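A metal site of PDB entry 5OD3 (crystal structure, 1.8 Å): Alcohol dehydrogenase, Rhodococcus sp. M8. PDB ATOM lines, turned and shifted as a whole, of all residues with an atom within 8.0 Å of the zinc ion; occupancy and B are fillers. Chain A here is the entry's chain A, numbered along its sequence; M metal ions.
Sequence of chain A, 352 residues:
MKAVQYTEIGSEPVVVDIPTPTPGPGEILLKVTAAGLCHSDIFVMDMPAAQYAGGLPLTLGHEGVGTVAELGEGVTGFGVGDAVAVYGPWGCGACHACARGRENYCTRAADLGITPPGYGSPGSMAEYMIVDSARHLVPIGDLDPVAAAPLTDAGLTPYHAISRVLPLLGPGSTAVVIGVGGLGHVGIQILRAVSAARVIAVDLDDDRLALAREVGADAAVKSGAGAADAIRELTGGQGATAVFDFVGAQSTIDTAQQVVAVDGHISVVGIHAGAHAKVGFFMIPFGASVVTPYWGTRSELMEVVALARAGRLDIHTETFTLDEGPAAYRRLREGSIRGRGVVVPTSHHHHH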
ATOM      1  N   TRP A  90     -21.718  -7.994 -13.175  1.00  0.00           N
ATOM      2  CA  TRP A  90     -22.653  -8.816 -13.918  1.00  0.00           C
ATOM      3  C   TRP A  90     -22.309 -10.298 -13.822  1.00  0.00           C
ATOM      4  O   TRP A  90     -21.137 -10.683 -13.954  1.00  0.00           O
ATOM      5  CB  TRP A  90     -22.686  -8.408 -15.424  1.00  0.00           C
ATOM      6  CG  TRP A  90     -23.126  -7.003 -15.669  1.00  0.00           C
ATOM      7  CD1 TRP A  90     -23.724  -6.150 -14.791  1.00  0.00           C
ATOM      8  CD2 TRP A  90     -23.059  -6.309 -16.917  1.00  0.00           C
ATOM      9  NE1 TRP A  90     -23.991  -4.952 -15.403  1.00  0.00           N
ATOM     10  CE2 TRP A  90     -23.596  -5.026 -16.705  1.00  0.00           C
ATOM     11  CE3 TRP A  90     -22.541  -6.640 -18.178  1.00  0.00           C
ATOM     12  CZ2 TRP A  90     -23.650  -4.053 -17.729  1.00  0.00           C
ATOM     13  CZ3 TRP A  90     -22.604  -5.687 -19.197  1.00  0.00           C
ATOM     14  CH2 TRP A  90     -23.140  -4.397 -18.955  1.00  0.00           C
ATOM     15  N   GLY A  91     -23.345 -11.087 -13.565  1.00  0.00           N
ATOM     16  CA  GLY A  91     -23.226 -12.545 -13.519  1.00  0.00           C
ATOM     17  C   GLY A  91     -24.115 -13.219 -14.546  1.00  0.00           C
ATOM     18  O   GLY A  91     -24.797 -12.552 -15.338  1.00  0.00           O
ATOM     19  N   CYS A  92     -24.155 -14.546 -14.470  1.00  0.00           N
ATOM     20  CA  CYS A  92     -24.876 -15.362 -15.423  1.00  0.00           C
ATOM     21  C   CYS A  92     -26.397 -15.293 -15.178  1.00  0.00           C
ATOM     22  O   CYS A  92     -27.170 -15.545 -16.082  1.00  0.00           O
ATOM     23  CB  CYS A  92     -24.379 -16.804 -15.346  1.00  0.00           C
ATOM     24  SG  CYS A  92     -24.968 -17.766 -13.927  1.00  0.00           S
ATOM     25  N   GLY A  93     -26.810 -14.977 -13.956  1.00  0.00           N
ATOM     26  CA  GLY A  93     -28.240 -14.852 -13.635  1.00  0.00           C
ATOM     27  C   GLY A  93     -28.966 -16.142 -13.287  1.00  0.00           C
ATOM     28  O   GLY A  93     -30.138 -16.108 -12.888  1.00  0.00           O
ATOM     29  N   ALA A  94     -28.273 -17.284 -13.430  1.00  0.00           N
ATOM     30  CA  ALA A  94     -28.903 -18.598 -13.393  1.00  0.00           C
ATOM     31  C   ALA A  94     -28.384 -19.547 -12.295  1.00  0.00           C
ATOM     32  O   ALA A  94     -29.093 -20.458 -11.907  1.00  0.00           O
ATOM     33  CB  ALA A  94     -28.756 -19.272 -14.742  1.00  0.00           C
ATOM     34  N   CYS A  95     -27.137 -19.354 -11.853  1.00  0.00           N
ATOM     35  CA  CYS A  95     -26.505 -20.183 -10.837  1.00  0.00           C
ATOM     36  C   CYS A  95     -27.072 -19.902  -9.445  1.00  0.00           C
ATOM     37  O   CYS A  95     -27.859 -18.969  -9.260  1.00  0.00           O
ATOM     38  CB  CYS A  95     -24.983 -19.965 -10.837  1.00  0.00           C
ATOM     39  SG  CYS A  95     -24.407 -18.391 -10.155  1.00  0.00           S
ATOM     40  N   HIS A  96     -26.689 -20.723  -8.488  1.00  0.00           N
ATOM     41  CA  HIS A  96     -27.185 -20.608  -7.116  1.00  0.00           C
ATOM     42  C   HIS A  96     -26.917 -19.225  -6.486  1.00  0.00           C
ATOM     43  O   HIS A  96     -27.798 -18.647  -5.832  1.00  0.00           O
ATOM     44  CB  HIS A  96     -26.593 -21.719  -6.258  1.00  0.00           C
ATOM     45  CG  HIS A  96     -27.184 -21.808  -4.885  1.00  0.00           C
ATOM     46  ND1 HIS A  96     -26.585 -21.228  -3.793  1.00  0.00           N
ATOM     47  CD2 HIS A  96     -28.299 -22.411  -4.421  1.00  0.00           C
ATOM     48  CE1 HIS A  96     -27.323 -21.465  -2.719  1.00  0.00           C
ATOM     49  NE2 HIS A  96     -28.361 -22.178  -3.072  1.00  0.00           N
ATOM     50  N   ALA A  97     -25.702 -18.710  -6.676  1.00  0.00           N
ATOM     51  CA  ALA A  97     -25.370 -17.363  -6.222  1.00  0.00           C
ATOM     52  C   ALA A  97     -26.225 -16.298  -6.931  1.00  0.00           C
ATOM     53  O   ALA A  97     -26.836 -15.450  -6.274  1.00  0.00           O
ATOM     54  CB  ALA A  97     -23.884 -17.091  -6.422  1.00  0.00           C
ATOM     55  N   CYS A  98     -26.327 -16.367  -8.267  1.00  0.00           N
ATOM     56  CA  CYS A  98     -27.089 -15.375  -9.015  1.00  0.00           C
ATOM     57  C   CYS A  98     -28.596 -15.418  -8.676  1.00  0.00           C
ATOM     58  O   CYS A  98     -29.241 -14.369  -8.643  1.00  0.00           O
ATOM     59  CB  CYS A  98     -26.902 -15.498 -10.547  1.00  0.00           C
ATOM     60  SG  CYS A  98     -25.277 -14.966 -11.119  1.00  0.00           S
ATOM     61  N   ALA A  99     -29.117 -16.607  -8.392  1.00  0.00           N
ATOM     62  CA  ALA A  99     -30.532 -16.762  -8.023  1.00  0.00           C
ATOM     63  C   ALA A  99     -30.881 -16.025  -6.728  1.00  0.00           C
ATOM     64  O   ALA A  99     -32.021 -15.608  -6.536  1.00  0.00           O
ATOM     65  CB  ALA A  99     -30.902 -18.227  -7.907  1.00  0.00           C
ATOM     66  N   ARG A 102     -26.731 -12.582  -5.899  1.00  0.00           N
ATOM     67  CA  ARG A 102     -25.331 -12.421  -5.476  1.00  0.00           C
ATOM     68  C   ARG A 102     -24.460 -12.595  -6.683  1.00  0.00           C
ATOM     69  O   ARG A 102     -23.626 -13.506  -6.739  1.00  0.00           O
ATOM     70  CB  ARG A 102     -24.965 -13.410  -4.359  1.00  0.00           C
ATOM     71  CG  ARG A 102     -25.869 -13.294  -3.144  1.00  0.00           C
ATOM     72  CD  ARG A 102     -25.644 -14.420  -2.140  1.00  0.00           C
ATOM     73  NE  ARG A 102     -24.351 -14.335  -1.489  1.00  0.00           N
ATOM     74  CZ  ARG A 102     -24.062 -13.519  -0.480  1.00  0.00           C
ATOM     75  NH1 ARG A 102     -24.960 -12.647  -0.015  1.00  0.00           N
ATOM     76  NH2 ARG A 102     -22.842 -13.515   0.042  1.00  0.00           N
ATOM     77  N   GLU A 103     -24.650 -11.734  -7.689  1.00  0.00           N
ATOM     78  CA  GLU A 103     -23.987 -11.925  -8.958  1.00  0.00           C
ATOM     79  C   GLU A 103     -22.497 -11.604  -8.861  1.00  0.00           C
ATOM     80  O   GLU A 103     -21.697 -12.089  -9.660  1.00  0.00           O
ATOM     81  CB  GLU A 103     -24.653 -11.133 -10.077  1.00  0.00           C
ATOM     82  CG  GLU A 103     -26.150 -11.436 -10.236  1.00  0.00           C
ATOM     83  CD  GLU A 103     -26.711 -11.098 -11.627  1.00  0.00           C
ATOM     84  OE1 GLU A 103     -25.952 -10.651 -12.522  1.00  0.00           O
ATOM     85  OE2 GLU A 103     -27.938 -11.299 -11.815  1.00  0.00           O
ATOM     86  N   ASN A 104     -22.138 -10.804  -7.855  1.00  0.00           N
ATOM     87  CA  ASN A 104     -20.736 -10.597  -7.484  1.00  0.00           C
ATOM     88  C   ASN A 104     -19.977 -11.921  -7.207  1.00  0.00           C
ATOM     89  O   ASN A 104     -18.752 -11.991  -7.405  1.00  0.00           O
ATOM     90  CB  ASN A 104     -20.600  -9.616  -6.298  1.00  0.00           C
ATOM     91  CG  ASN A 104     -21.409 -10.005  -5.061  1.00  0.00           C
ATOM     92  OD1 ASN A 104     -22.502 -10.589  -5.172  1.00  0.00           O
ATOM     93  ND2 ASN A 104     -20.884  -9.662  -3.880  1.00  0.00           N
ATOM     94  N   TYR A 105     -20.685 -12.931  -6.751  1.00  0.00           N
ATOM     95  CA  TYR A 105     -20.095 -14.243  -6.456  1.00  0.00           C
ATOM     96  C   TYR A 105     -20.552 -15.310  -7.440  1.00  0.00           C
ATOM     97  O   TYR A 105     -20.542 -16.516  -7.117  1.00  0.00           O
ATOM     98  CB  TYR A 105     -20.403 -14.637  -5.000  1.00  0.00           C
ATOM     99  CG  TYR A 105     -19.844 -13.653  -3.976  1.00  0.00           C
ATOM    100  CD1 TYR A 105     -18.521 -13.241  -4.038  1.00  0.00           C
ATOM    101  CD2 TYR A 105     -20.619 -13.198  -2.919  1.00  0.00           C
ATOM    102  CE1 TYR A 105     -18.001 -12.345  -3.109  1.00  0.00           C
ATOM    103  CE2 TYR A 105     -20.092 -12.315  -1.970  1.00  0.00           C
ATOM    104  CZ  TYR A 105     -18.776 -11.886  -2.093  1.00  0.00           C
ATOM    105  OH  TYR A 105     -18.236 -11.011  -1.174  1.00  0.00           O
ATOM    106  N   CYS A 106     -20.903 -14.887  -8.654  1.00  0.00           N
ATOM    107  CA  CYS A 106     -21.308 -15.810  -9.709  1.00  0.00           C
ATOM    108  C   CYS A 106     -20.164 -16.760 -10.009  1.00  0.00           C
ATOM    109  O   CYS A 106     -19.055 -16.329 -10.179  1.00  0.00           O
ATOM    110  CB  CYS A 106     -21.612 -15.039 -11.007  1.00  0.00           C
ATOM    111  SG  CYS A 106     -22.067 -16.148 -12.352  1.00  0.00           S
ATOM    112  N   THR A 107     -20.483 -18.057 -10.089  1.00  0.00           N
ATOM    113  CA  THR A 107     -19.503 -19.122 -10.327  1.00  0.00           C
ATOM    114  C   THR A 107     -19.296 -19.443 -11.817  1.00  0.00           C
ATOM    115  O   THR A 107     -18.431 -20.246 -12.146  1.00  0.00           O
ATOM    116  CB  THR A 107     -19.950 -20.415  -9.600  1.00  0.00           C
ATOM    117  OG1 THR A 107     -21.358 -20.648  -9.824  1.00  0.00           O
ATOM    118  CG2 THR A 107     -19.747 -20.291  -8.096  1.00  0.00           C
ATOM    119  N   ARG A 108     -20.084 -18.828 -12.698  1.00  0.00           N
ATOM    120  CA  ARG A 108     -20.079 -19.118 -14.131  1.00  0.00           C
ATOM    121  C   ARG A 108     -19.647 -17.966 -15.043  1.00  0.00           C
ATOM    122  O   ARG A 108     -19.474 -18.182 -16.258  1.00  0.00           O
ATOM    123  CB  ARG A 108     -21.488 -19.573 -14.542  1.00  0.00           C
ATOM    124  CG  ARG A 108     -21.943 -20.908 -13.976  1.00  0.00           C
ATOM    125  CD  ARG A 108     -23.229 -21.344 -14.658  1.00  0.00           C
ATOM    126  NE  ARG A 108     -24.115 -22.131 -13.784  1.00  0.00           N
ATOM    127  CZ  ARG A 108     -25.428 -22.334 -13.984  1.00  0.00           C
ATOM    128  NH1 ARG A 108     -26.110 -23.059 -13.106  1.00  0.00           N
ATOM    129  NH2 ARG A 108     -26.064 -21.804 -15.040  1.00  0.00           N
ATOM    130  N   ALA A 109     -19.459 -16.769 -14.496  1.00  0.00           N
ATOM    131  CA  ALA A 109     -19.226 -15.560 -15.307  1.00  0.00           C
ATOM    132  C   ALA A 109     -17.934 -15.662 -16.107  1.00  0.00           C
ATOM    133  O   ALA A 109     -17.933 -15.371 -17.305  1.00  0.00           O
ATOM    134  CB  ALA A 109     -19.217 -14.293 -14.429  1.00  0.00           C
ATOM    135  N   LEU A 112     -18.332 -18.127 -19.044  1.00  0.00           N
ATOM    136  CA  LEU A 112     -19.207 -17.570 -20.079  1.00  0.00           C
ATOM    137  C   LEU A 112     -18.710 -16.235 -20.674  1.00  0.00           C
ATOM    138  O   LEU A 112     -19.389 -15.672 -21.534  1.00  0.00           O
ATOM    139  CB  LEU A 112     -20.627 -17.401 -19.526  1.00  0.00           C
ATOM    140  CG  LEU A 112     -21.365 -18.678 -19.092  1.00  0.00           C
ATOM    141  CD1 LEU A 112     -22.630 -18.313 -18.328  1.00  0.00           C
ATOM    142  CD2 LEU A 112     -21.691 -19.540 -20.305  1.00  0.00           C
ATOM    143  N   ILE A 114     -18.497 -13.250 -19.135  1.00  0.00           N
ATOM    144  CA  ILE A 114     -19.318 -12.130 -18.687  1.00  0.00           C
ATOM    145  C   ILE A 114     -18.440 -11.256 -17.830  1.00  0.00           C
ATOM    146  O   ILE A 114     -17.916 -11.681 -16.810  1.00  0.00           O
ATOM    147  CB  ILE A 114     -20.576 -12.575 -17.897  1.00  0.00           C
ATOM    148  CG1 ILE A 114     -21.515 -13.389 -18.796  1.00  0.00           C
ATOM    149  CG2 ILE A 114     -21.325 -11.370 -17.362  1.00  0.00           C
ATOM    150  CD1 ILE A 114     -22.548 -14.203 -18.037  1.00  0.00           C
ATOM    151  N   ARG A 135     -32.373  -6.582 -15.369  1.00  0.00           N
ATOM    152  CA  ARG A 135     -32.066  -6.901 -13.958  1.00  0.00           C
ATOM    153  C   ARG A 135     -30.812  -6.205 -13.425  1.00  0.00           C
ATOM    154  O   ARG A 135     -30.572  -6.235 -12.209  1.00  0.00           O
ATOM    155  CB  ARG A 135     -32.005  -8.414 -13.733  1.00  0.00           C
ATOM    156  CG  ARG A 135     -30.706  -9.083 -14.139  1.00  0.00           C
ATOM    157  CD  ARG A 135     -30.723 -10.599 -13.921  1.00  0.00           C
ATOM    158  NE  ARG A 135     -29.362 -11.108 -14.083  1.00  0.00           N
ATOM    159  CZ  ARG A 135     -28.797 -11.392 -15.254  1.00  0.00           C
ATOM    160  NH1 ARG A 135     -29.457 -11.222 -16.413  1.00  0.00           N
ATOM    161  NH2 ARG A 135     -27.541 -11.826 -15.279  1.00  0.00           N
HETATM  162 ZN    ZN M   1     -24.181 -16.887 -11.922  1.00  0.00          ZN
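The side-chain sulfur of Cys 92 lies close to the backbone NH of Ala 94 (3.4 Å). The side-chain sulfur of Cys 106 sits close to the backbone NH of Arg 108, at 3.4 Å. SG of Cys 106 lies close to N of Ala 109 (3.4 Å). The side-chain sulfur (SG) of Cys 98 sits close to the backbone NH (N) of Gly 93, 3.2 Å away. N of Ala 97 lies close to SG of Cys 95.
N of Gly 93 touches the zinc ion, 3.8 Å away. Five residues have an atom within 4 Å of the zinc ion: Cys 92, Gly 93, Cys 95, Cys 98 and Cys 106.
The side-chain sulfur (SG) of Cys 106 binds the zinc ion. The zinc ion is bound by SG of Cys 92, 2.3 Å away. SG of Cys 95 is bound to the zinc ion (2.3 Å). The side-chain sulfur (SG) of Cys 98 is bound to the zinc ion.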
